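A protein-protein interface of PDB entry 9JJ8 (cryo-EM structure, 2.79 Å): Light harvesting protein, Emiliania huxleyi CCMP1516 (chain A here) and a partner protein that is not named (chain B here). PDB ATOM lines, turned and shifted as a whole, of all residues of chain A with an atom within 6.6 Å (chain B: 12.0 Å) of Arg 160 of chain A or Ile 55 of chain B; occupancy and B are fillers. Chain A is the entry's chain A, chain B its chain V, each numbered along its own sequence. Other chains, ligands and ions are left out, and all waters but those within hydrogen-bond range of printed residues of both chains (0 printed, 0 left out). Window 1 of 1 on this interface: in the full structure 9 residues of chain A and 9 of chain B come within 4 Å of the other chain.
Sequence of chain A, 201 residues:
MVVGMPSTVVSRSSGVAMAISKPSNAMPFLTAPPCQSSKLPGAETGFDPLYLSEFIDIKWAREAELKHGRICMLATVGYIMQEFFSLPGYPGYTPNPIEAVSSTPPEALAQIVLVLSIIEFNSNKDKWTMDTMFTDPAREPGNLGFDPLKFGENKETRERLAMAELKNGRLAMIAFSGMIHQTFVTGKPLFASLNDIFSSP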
ATOM      1  N   PHE A 151      17.416  23.043 -25.827  1.00  0.00           N
ATOM      2  CA  PHE A 151      17.713  21.629 -26.023  1.00  0.00           C
ATOM      3  C   PHE A 151      19.081  21.438 -26.660  1.00  0.00           C
ATOM      4  O   PHE A 151      19.798  20.489 -26.325  1.00  0.00           O
ATOM      5  CB  PHE A 151      16.646  20.981 -26.902  1.00  0.00           C
ATOM      6  CG  PHE A 151      15.373  20.654 -26.184  1.00  0.00           C
ATOM      7  CD1 PHE A 151      14.381  21.607 -26.036  1.00  0.00           C
ATOM      8  CD2 PHE A 151      15.143  19.374 -25.712  1.00  0.00           C
ATOM      9  CE1 PHE A 151      13.199  21.299 -25.394  1.00  0.00           C
ATOM     10  CE2 PHE A 151      13.964  19.060 -25.067  1.00  0.00           C
ATOM     11  CZ  PHE A 151      12.992  20.024 -24.912  1.00  0.00           C
ATOM     12  N   GLY A 152      19.458  22.330 -27.574  1.00  0.00           N
ATOM     13  CA  GLY A 152      20.687  22.260 -28.332  1.00  0.00           C
ATOM     14  C   GLY A 152      21.940  22.689 -27.608  1.00  0.00           C
ATOM     15  O   GLY A 152      22.952  22.953 -28.260  1.00  0.00           O
ATOM     16  N   ASN A 154      22.983  20.594 -25.135  1.00  0.00           N
ATOM     17  CA  ASN A 154      23.392  19.331 -24.529  1.00  0.00           C
ATOM     18  C   ASN A 154      24.622  18.758 -25.225  1.00  0.00           C
ATOM     19  O   ASN A 154      25.627  18.470 -24.567  1.00  0.00           O
ATOM     20  CB  ASN A 154      22.233  18.334 -24.573  1.00  0.00           C
ATOM     21  CG  ASN A 154      22.417  17.181 -23.609  1.00  0.00           C
ATOM     22  OD1 ASN A 154      23.259  17.234 -22.712  1.00  0.00           O
ATOM     23  ND2 ASN A 154      21.624  16.132 -23.783  1.00  0.00           N
ATOM     24  N   GLU A 156      25.056  15.863 -26.612  1.00  0.00           N
ATOM     25  CA  GLU A 156      25.039  14.412 -26.781  1.00  0.00           C
ATOM     26  C   GLU A 156      23.795  13.924 -27.507  1.00  0.00           C
ATOM     27  O   GLU A 156      23.881  13.000 -28.321  1.00  0.00           O
ATOM     28  CB  GLU A 156      25.151  13.670 -25.440  1.00  0.00           C
ATOM     29  CG  GLU A 156      26.482  13.818 -24.713  1.00  0.00           C
ATOM     30  CD  GLU A 156      26.570  15.084 -23.898  1.00  0.00           C
ATOM     31  OE1 GLU A 156      25.564  15.814 -23.846  1.00  0.00           O
ATOM     32  OE2 GLU A 156      27.641  15.348 -23.312  1.00  0.00           O
ATOM     33  N   THR A 157      22.641  14.525 -27.233  1.00  0.00           N
ATOM     34  CA  THR A 157      21.399  14.183 -27.909  1.00  0.00           C
ATOM     35  C   THR A 157      21.094  15.101 -29.082  1.00  0.00           C
ATOM     36  O   THR A 157      19.989  15.035 -29.632  1.00  0.00           O
ATOM     37  CB  THR A 157      20.234  14.202 -26.917  1.00  0.00           C
ATOM     38  OG1 THR A 157      20.191  15.468 -26.247  1.00  0.00           O
ATOM     39  CG2 THR A 157      20.395  13.087 -25.907  1.00  0.00           C
ATOM     40  N   ARG A 158      22.047  15.953 -29.471  1.00  0.00           N
ATOM     41  CA  ARG A 158      21.854  16.828 -30.623  1.00  0.00           C
ATOM     42  C   ARG A 158      21.666  16.023 -31.902  1.00  0.00           C
ATOM     43  O   ARG A 158      20.778  16.319 -32.712  1.00  0.00           O
ATOM     44  CB  ARG A 158      23.046  17.777 -30.754  1.00  0.00           C
ATOM     45  CG  ARG A 158      23.030  18.635 -32.006  1.00  0.00           C
ATOM     46  CD  ARG A 158      21.935  19.681 -31.948  1.00  0.00           C
ATOM     47  NE  ARG A 158      21.846  20.439 -33.191  1.00  0.00           N
ATOM     48  CZ  ARG A 158      21.093  21.516 -33.357  1.00  0.00           C
ATOM     49  NH1 ARG A 158      20.358  22.004 -32.371  1.00  0.00           N
ATOM     50  NH2 ARG A 158      21.079  22.121 -34.541  1.00  0.00           N
ATOM     51  N   GLU A 159      22.479  14.978 -32.086  1.00  0.00           N
ATOM     52  CA  GLU A 159      22.390  14.172 -33.299  1.00  0.00           C
ATOM     53  C   GLU A 159      21.091  13.376 -33.352  1.00  0.00           C
ATOM     54  O   GLU A 159      20.444  13.305 -34.406  1.00  0.00           O
ATOM     55  CB  GLU A 159      23.595  13.236 -33.394  1.00  0.00           C
ATOM     56  CG  GLU A 159      23.612  12.376 -34.646  1.00  0.00           C
ATOM     57  CD  GLU A 159      23.729  13.195 -35.918  1.00  0.00           C
ATOM     58  OE1 GLU A 159      24.420  14.237 -35.899  1.00  0.00           O
ATOM     59  OE2 GLU A 159      23.126  12.799 -36.937  1.00  0.00           O
ATOM     60  N   ARG A 160      20.684  12.784 -32.226  1.00  0.00           N
ATOM     61  CA  ARG A 160      19.450  12.006 -32.224  1.00  0.00           C
ATOM     62  C   ARG A 160      18.231  12.911 -32.363  1.00  0.00           C
ATOM     63  O   ARG A 160      17.244  12.527 -32.996  1.00  0.00           O
ATOM     64  CB  ARG A 160      19.362  11.130 -30.968  1.00  0.00           C
ATOM     65  CG  ARG A 160      19.084  11.855 -29.662  1.00  0.00           C
ATOM     66  CD  ARG A 160      18.431  10.938 -28.642  1.00  0.00           C
ATOM     67  NE  ARG A 160      17.034  10.678 -28.963  1.00  0.00           N
ATOM     68  CZ  ARG A 160      16.094  10.426 -28.063  1.00  0.00           C
ATOM     69  NH1 ARG A 160      16.365  10.406 -26.770  1.00  0.00           N
ATOM     70  NH2 ARG A 160      14.850  10.190 -28.472  1.00  0.00           N
ATOM     71  N   LEU A 161      18.301  14.137 -31.833  1.00  0.00           N
ATOM     72  CA  LEU A 161      17.197  15.074 -32.019  1.00  0.00           C
ATOM     73  C   LEU A 161      17.123  15.563 -33.461  1.00  0.00           C
ATOM     74  O   LEU A 161      16.025  15.738 -34.002  1.00  0.00           O
ATOM     75  CB  LEU A 161      17.332  16.247 -31.049  1.00  0.00           C
ATOM     76  CG  LEU A 161      16.817  15.984 -29.631  1.00  0.00           C
ATOM     77  CD1 LEU A 161      17.112  17.158 -28.714  1.00  0.00           C
ATOM     78  CD2 LEU A 161      15.330  15.675 -29.651  1.00  0.00           C
ATOM     79  N   ALA A 162      18.278  15.770 -34.104  1.00  0.00           N
ATOM     80  CA  ALA A 162      18.289  16.161 -35.511  1.00  0.00           C
ATOM     81  C   ALA A 162      17.720  15.058 -36.396  1.00  0.00           C
ATOM     82  O   ALA A 162      16.912  15.322 -37.297  1.00  0.00           O
ATOM     83  CB  ALA A 162      19.710  16.519 -35.941  1.00  0.00           C
ATOM     84  N   MET A 163      18.117  13.809 -36.138  1.00  0.00           N
ATOM     85  CA  MET A 163      17.583  12.691 -36.911  1.00  0.00           C
ATOM     86  C   MET A 163      16.096  12.490 -36.649  1.00  0.00           C
ATOM     87  O   MET A 163      15.341  12.163 -37.574  1.00  0.00           O
ATOM     88  CB  MET A 163      18.362  11.413 -36.606  1.00  0.00           C
ATOM     89  CG  MET A 163      19.807  11.456 -37.060  1.00  0.00           C
ATOM     90  SD  MET A 163      19.931  11.680 -38.844  1.00  0.00           S
ATOM     91  CE  MET A 163      19.315  10.103 -39.424  1.00  0.00           C
ATOM     92  N   ALA A 164      15.657  12.685 -35.401  1.00  0.00           N
ATOM     93  CA  ALA A 164      14.237  12.580 -35.083  1.00  0.00           C
ATOM     94  C   ALA A 164      13.431  13.642 -35.816  1.00  0.00           C
ATOM     95  O   ALA A 164      12.378  13.343 -36.390  1.00  0.00           O
ATOM     96  CB  ALA A 164      14.030  12.689 -33.572  1.00  0.00           C
ATOM     97  N   GLU A 165      13.934  14.882 -35.837  1.00  0.00           N
ATOM     98  CA  GLU A 165      13.251  15.957 -36.552  1.00  0.00           C
ATOM     99  C   GLU A 165      13.173  15.661 -38.044  1.00  0.00           C
ATOM    100  O   GLU A 165      12.118  15.829 -38.664  1.00  0.00           O
ATOM    101  CB  GLU A 165      13.962  17.291 -36.328  1.00  0.00           C
ATOM    102  CG  GLU A 165      13.400  18.409 -37.206  1.00  0.00           C
ATOM    103  CD  GLU A 165      14.155  19.712 -37.088  1.00  0.00           C
ATOM    104  OE1 GLU A 165      15.113  19.782 -36.299  1.00  0.00           O
ATOM    105  OE2 GLU A 165      13.784  20.673 -37.790  1.00  0.00           O
ATOM    106  N   VAL B  32      20.121  13.210 -14.982  1.00  0.00           N
ATOM    107  CA  VAL B  32      18.771  12.926 -14.526  1.00  0.00           C
ATOM    108  C   VAL B  32      18.476  14.079 -13.559  1.00  0.00           C
ATOM    109  O   VAL B  32      19.412  14.761 -13.141  1.00  0.00           O
ATOM    110  CB  VAL B  32      18.689  11.504 -13.894  1.00  0.00           C
ATOM    111  CG1 VAL B  32      17.296  11.162 -13.383  1.00  0.00           C
ATOM    112  CG2 VAL B  32      19.160  10.456 -14.891  1.00  0.00           C
ATOM    113  N   SER B  33      17.201  14.337 -13.243  1.00  0.00           N
ATOM    114  CA  SER B  33      16.824  15.445 -12.371  1.00  0.00           C
ATOM    115  C   SER B  33      17.442  15.312 -10.982  1.00  0.00           C
ATOM    116  O   SER B  33      18.333  16.093 -10.632  1.00  0.00           O
ATOM    117  CB  SER B  33      15.301  15.529 -12.260  1.00  0.00           C
ATOM    118  OG  SER B  33      14.706  15.737 -13.528  1.00  0.00           O
ATOM    119  N   ASP B  48      10.595   8.780 -14.457  1.00  0.00           N
ATOM    120  CA  ASP B  48      10.953   9.095 -15.839  1.00  0.00           C
ATOM    121  C   ASP B  48      10.747   7.865 -16.714  1.00  0.00           C
ATOM    122  O   ASP B  48      11.708   7.154 -17.037  1.00  0.00           O
ATOM    123  CB  ASP B  48      12.397   9.591 -15.925  1.00  0.00           C
ATOM    124  CG  ASP B  48      12.537  11.044 -15.530  1.00  0.00           C
ATOM    125  OD1 ASP B  48      11.548  11.791 -15.666  1.00  0.00           O
ATOM    126  OD2 ASP B  48      13.636  11.443 -15.091  1.00  0.00           O
ATOM    127  N   PRO B  49       9.493   7.565 -17.101  1.00  0.00           N
ATOM    128  CA  PRO B  49       9.257   6.451 -18.034  1.00  0.00           C
ATOM    129  C   PRO B  49       9.846   6.714 -19.410  1.00  0.00           C
ATOM    130  O   PRO B  49      10.676   5.945 -19.907  1.00  0.00           O
ATOM    131  CB  PRO B  49       7.727   6.361 -18.097  1.00  0.00           C
ATOM    132  CG  PRO B  49       7.231   7.133 -16.923  1.00  0.00           C
ATOM    133  CD  PRO B  49       8.235   8.212 -16.700  1.00  0.00           C
ATOM    134  N   MET B  50       9.415   7.812 -20.026  1.00  0.00           N
ATOM    135  CA  MET B  50       9.991   8.322 -21.262  1.00  0.00           C
ATOM    136  C   MET B  50      11.288   9.072 -21.031  1.00  0.00           C
ATOM    137  O   MET B  50      11.989   9.393 -21.995  1.00  0.00           O
ATOM    138  CB  MET B  50       9.002   9.259 -21.956  1.00  0.00           C
ATOM    139  CG  MET B  50       7.721   8.646 -22.469  1.00  0.00           C
ATOM    140  SD  MET B  50       8.043   7.404 -23.724  1.00  0.00           S
ATOM    141  CE  MET B  50       7.823   5.896 -22.799  1.00  0.00           C
ATOM    142  N   GLY B  51      11.613   9.353 -19.780  1.00  0.00           N
ATOM    143  CA  GLY B  51      12.690  10.253 -19.458  1.00  0.00           C
ATOM    144  C   GLY B  51      12.246  11.699 -19.498  1.00  0.00           C
ATOM    145  O   GLY B  51      12.037  12.307 -18.445  1.00  0.00           O
ATOM    146  N   LEU B  52      12.154  12.269 -20.712  1.00  0.00           N
ATOM    147  CA  LEU B  52      11.922  13.693 -20.992  1.00  0.00           C
ATOM    148  C   LEU B  52      13.038  14.594 -20.463  1.00  0.00           C
ATOM    149  O   LEU B  52      13.037  15.802 -20.711  1.00  0.00           O
ATOM    150  CB  LEU B  52      10.567  14.178 -20.462  1.00  0.00           C
ATOM    151  CG  LEU B  52       9.338  14.188 -21.377  1.00  0.00           C
ATOM    152  CD1 LEU B  52       9.559  15.168 -22.518  1.00  0.00           C
ATOM    153  CD2 LEU B  52       9.015  12.831 -21.924  1.00  0.00           C
ATOM    154  N   SER B  53      14.001  14.010 -19.767  1.00  0.00           N
ATOM    155  CA  SER B  53      15.253  14.603 -19.352  1.00  0.00           C
ATOM    156  C   SER B  53      16.359  13.846 -20.066  1.00  0.00           C
ATOM    157  O   SER B  53      16.110  12.824 -20.712  1.00  0.00           O
ATOM    158  CB  SER B  53      15.415  14.536 -17.832  1.00  0.00           C
ATOM    159  OG  SER B  53      16.723  14.914 -17.445  1.00  0.00           O
ATOM    160  N   LYS B  54      17.575  14.392 -19.997  1.00  0.00           N
ATOM    161  CA  LYS B  54      18.799  13.899 -20.629  1.00  0.00           C
ATOM    162  C   LYS B  54      18.759  13.990 -22.151  1.00  0.00           C
ATOM    163  O   LYS B  54      19.776  13.718 -22.793  1.00  0.00           O
ATOM    164  CB  LYS B  54      19.145  12.457 -20.222  1.00  0.00           C
ATOM    165  CG  LYS B  54      19.290  12.273 -18.730  1.00  0.00           C
ATOM    166  CD  LYS B  54      20.498  13.028 -18.226  1.00  0.00           C
ATOM    167  CE  LYS B  54      21.776  12.296 -18.577  1.00  0.00           C
ATOM    168  NZ  LYS B  54      21.872  11.008 -17.835  1.00  0.00           N
ATOM    169  N   ILE B  55      17.627  14.372 -22.747  1.00  0.00           N
ATOM    170  CA  ILE B  55      17.562  14.791 -24.138  1.00  0.00           C
ATOM    171  C   ILE B  55      17.787  16.281 -24.278  1.00  0.00           C
ATOM    172  O   ILE B  55      17.719  16.817 -25.393  1.00  0.00           O
ATOM    173  CB  ILE B  55      16.213  14.402 -24.773  1.00  0.00           C
ATOM    174  CG1 ILE B  55      15.078  15.219 -24.157  1.00  0.00           C
ATOM    175  CG2 ILE B  55      15.941  12.924 -24.577  1.00  0.00           C
ATOM    176  CD1 ILE B  55      13.755  15.061 -24.870  1.00  0.00           C
ATOM    177  N   ALA B  56      18.055  16.968 -23.171  1.00  0.00           N
ATOM    178  CA  ALA B  56      18.134  18.418 -23.132  1.00  0.00           C
ATOM    179  C   ALA B  56      19.295  18.868 -22.257  1.00  0.00           C
ATOM    180  O   ALA B  56      20.056  18.038 -21.752  1.00  0.00           O
ATOM    181  CB  ALA B  56      16.821  18.992 -22.612  1.00  0.00           C
ATOM    182  N   SER B  57      19.429  20.175 -22.058  1.00  0.00           N
ATOM    183  CA  SER B  57      20.503  20.732 -21.257  1.00  0.00           C
ATOM    184  C   SER B  57      20.052  20.886 -19.806  1.00  0.00           C
ATOM    185  O   SER B  57      18.946  20.498 -19.424  1.00  0.00           O
ATOM    186  CB  SER B  57      20.964  22.069 -21.837  1.00  0.00           C
ATOM    187  OG  SER B  57      19.856  22.897 -22.134  1.00  0.00           O
ATOM    188  N   ALA B  58      20.936  21.460 -18.987  1.00  0.00           N
ATOM    189  CA  ALA B  58      20.635  21.631 -17.570  1.00  0.00           C
ATOM    190  C   ALA B  58      19.582  22.710 -17.348  1.00  0.00           C
ATOM    191  O   ALA B  58      18.783  22.624 -16.409  1.00  0.00           O
ATOM    192  CB  ALA B  58      21.913  21.961 -16.799  1.00  0.00           C
ATOM    193  N   GLU B  59      19.572  23.741 -18.197  1.00  0.00           N
ATOM    194  CA  GLU B  59      18.613  24.829 -18.034  1.00  0.00           C
ATOM    195  C   GLU B  59      17.202  24.408 -18.422  1.00  0.00           C
ATOM    196  O   GLU B  59      16.225  24.966 -17.907  1.00  0.00           O
ATOM    197  CB  GLU B  59      19.053  26.041 -18.854  1.00  0.00           C
ATOM    198  CG  GLU B  59      19.321  25.743 -20.320  1.00  0.00           C
ATOM    199  CD  GLU B  59      20.786  25.459 -20.603  1.00  0.00           C
ATOM    200  OE1 GLU B  59      21.561  25.294 -19.637  1.00  0.00           O
ATOM    201  OE2 GLU B  59      21.159  25.396 -21.793  1.00  0.00           O
ATOM    202  N   THR B  60      17.073  23.428 -19.318  1.00  0.00           N
ATOM    203  CA  THR B  60      15.750  22.952 -19.702  1.00  0.00           C
ATOM    204  C   THR B  60      15.078  22.204 -18.554  1.00  0.00           C
ATOM    205  O   THR B  60      13.853  22.256 -18.417  1.00  0.00           O
ATOM    206  CB  THR B  60      15.864  22.072 -20.948  1.00  0.00           C
ATOM    207  OG1 THR B  60      16.539  22.801 -21.980  1.00  0.00           O
ATOM    208  CG2 THR B  60      14.492  21.678 -21.476  1.00  0.00           C
ATOM    209  N   LEU B  61      15.861  21.537 -17.701  1.00  0.00           N
ATOM    210  CA  LEU B  61      15.303  20.927 -16.495  1.00  0.00           C
ATOM    211  C   LEU B  61      14.755  21.976 -15.535  1.00  0.00           C
ATOM    212  O   LEU B  61      13.691  21.784 -14.931  1.00  0.00           O
ATOM    213  CB  LEU B  61      16.362  20.078 -15.796  1.00  0.00           C
ATOM    214  CG  LEU B  61      16.724  18.785 -16.511  1.00  0.00           C
ATOM    215  CD1 LEU B  61      17.887  18.091 -15.826  1.00  0.00           C
ATOM    216  CD2 LEU B  61      15.499  17.904 -16.512  1.00  0.00           C
ATOM    217  N   ALA B  62      15.474  23.087 -15.370  1.00  0.00           N
ATOM    218  CA  ALA B  62      14.986  24.161 -14.513  1.00  0.00           C
ATOM    219  C   ALA B  62      13.745  24.815 -15.107  1.00  0.00           C
ATOM    220  O   ALA B  62      12.827  25.200 -14.373  1.00  0.00           O
ATOM    221  CB  ALA B  62      16.088  25.190 -14.288  1.00  0.00           C
ATOM    222  N   TRP B  63      13.698  24.934 -16.436  1.00  0.00           N
ATOM    223  CA  TRP B  63      12.484  25.411 -17.093  1.00  0.00           C
ATOM    224  C   TRP B  63      11.325  24.444 -16.880  1.00  0.00           C
ATOM    225  O   TRP B  63      10.179  24.869 -16.688  1.00  0.00           O
ATOM    226  CB  TRP B  63      12.731  25.611 -18.586  1.00  0.00           C
ATOM    227  CG  TRP B  63      11.741  26.533 -19.205  1.00  0.00           C
ATOM    228  CD1 TRP B  63      11.797  27.894 -19.241  1.00  0.00           C
ATOM    229  CD2 TRP B  63      10.506  26.167 -19.823  1.00  0.00           C
ATOM    230  NE1 TRP B  63      10.691  28.398 -19.876  1.00  0.00           N
ATOM    231  CE2 TRP B  63       9.881  27.357 -20.242  1.00  0.00           C
ATOM    232  CE3 TRP B  63       9.874  24.949 -20.077  1.00  0.00           C
ATOM    233  CZ2 TRP B  63       8.657  27.363 -20.895  1.00  0.00           C
ATOM    234  CZ3 TRP B  63       8.660  24.959 -20.728  1.00  0.00           C
ATOM    235  CH2 TRP B  63       8.065  26.156 -21.128  1.00  0.00           C
ATOM    236  N   TYR B  64      11.609  23.137 -16.918  1.00  0.00           N
ATOM    237  CA  TYR B  64      10.590  22.128 -16.648  1.00  0.00           C
ATOM    238  C   TYR B  64      10.048  22.258 -15.233  1.00  0.00           C
ATOM    239  O   TYR B  64       8.838  22.151 -15.014  1.00  0.00           O
ATOM    240  CB  TYR B  64      11.165  20.725 -16.842  1.00  0.00           C
ATOM    241  CG  TYR B  64      11.353  20.283 -18.273  1.00  0.00           C
ATOM    242  CD1 TYR B  64      10.949  21.079 -19.333  1.00  0.00           C
ATOM    243  CD2 TYR B  64      11.915  19.049 -18.559  1.00  0.00           C
ATOM    244  CE1 TYR B  64      11.115  20.663 -20.640  1.00  0.00           C
ATOM    245  CE2 TYR B  64      12.084  18.629 -19.856  1.00  0.00           C
ATOM    246  CZ  TYR B  64      11.683  19.436 -20.892  1.00  0.00           C
ATOM    247  OH  TYR B  64      11.853  19.006 -22.184  1.00  0.00           O
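ND2 of Asn 154 of chain A lies within hydrogen-bond range of O of Lys 54 of chain B. The backbone carbonyl oxygen (O) of Ala 56 of chain B lies close to the side-chain amide nitrogen (ND2) of Asn 154 of chain A (3.2 Å). The side-chain hydroxyl (OG1) of Thr 157 of chain A lies within hydrogen-bond range of the backbone carbonyl oxygen (O) of Ile 55 of chain B (2.9 Å).
OD1 of Asn 154 of chain A lies close to OE1 of Glu 156 of chain A (2.9 Å). OG1 of Thr 157 of chain A lies within hydrogen-bond range of ND2 of Asn 154 of chain A, 2.9 Å away. OG1 of Thr 60 of chain B is in hydrogen-bond range of OG of Ser 57 of chain B (3.3 Å).
Among the printed residues, pairs that only touch across the chains: Phe 151 of chain A with Tyr 64 of chain B, Thr 157 of chain A with Lys 54 of chain B, Arg 160 of chain A with Ile 55 of chain B, Leu 161 of chain A with Ile 55 of chain B, Phe 151 of chain A with Ala 56 of chain B, Phe 151 of chain A with Ile 55 of chain B, Asn 154 of chain A with Ile 55 of chain B and Phe 151 of chain A with Thr 60 of chain B.
Of the printed residues of chain B, Arg 160 of chain A touches Ile 55. Of chain A, only Phe 151, Asn 154, Thr 157, Arg 160 and Leu 161 come within 4 Å of Ile 55 of chain B. Of chain B, only Ile 55, Ala 56, Thr 60 and Tyr 64 come within 4 Å of Phe 151 of chain A. Of chain B, only Lys 54 (3.2 Å) and Ile 55 (2.9 Å) come within 4 Å of Thr 157 of chain A. Of chain B, only Ile 55 (3.4 Å) comes within 4 Å of Leu 161 of chain A. No residue of chain B comes within 4 Å of Ala 162 of chain A. Met 163 of chain A touches none of the printed residues of chain B. Printed residues of chain A within 4 Å of Lys 54 of chain B: Asn 154 (3.2 Å) and Thr 157 (3.2 Å). Printed residues of chain A within 4 Å of Thr 60 of chain B: Phe 151 (3.95 Å). Val 32 of chain B touches none of the printed residues of chain A. Ser 53 of chain B touches none of the printed residues of chain A. The nearest residue of chain B that does not touch Arg 160 of chain A is Lys 54 of chain B (6.2 Å). The nearest residue of chain A that does not touch Ile 55 of chain B is Arg 158 of chain A (6.0 Å). The nearest printed residue of chain B that does not touch Asn 154 of chain A is Ser 57 of chain B (4.1 Å).
Of the 13 printed residues of chain A, 5 touch a printed residue of chain B. Printed residues of chain A that touch a printed residue of chain B: Phe 151, Asn 154, Thr 157, Arg 160 and Leu 161. Hydrophobic or aromatic side chains of chain A within 4 Å of the printed part of chain B: Phe 151 and Leu 161. Along chain A the printed residues that touch a printed residue of chain B span positions 151 to 161. Of the 19 printed residues of chain B, 5 touch a printed residue of chain A. Hydrophobic or aromatic side chains of chain B that line the printed part of chain A: Ile 55, Ala 56 and Tyr 64. Along chain B the printed residues that touch a printed residue of chain A span positions 54 to 64. Among the printed residues, no Asp or Glu carboxylate lies within 4 Å of a Lys or Arg side-chain nitrogen of the other chain.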
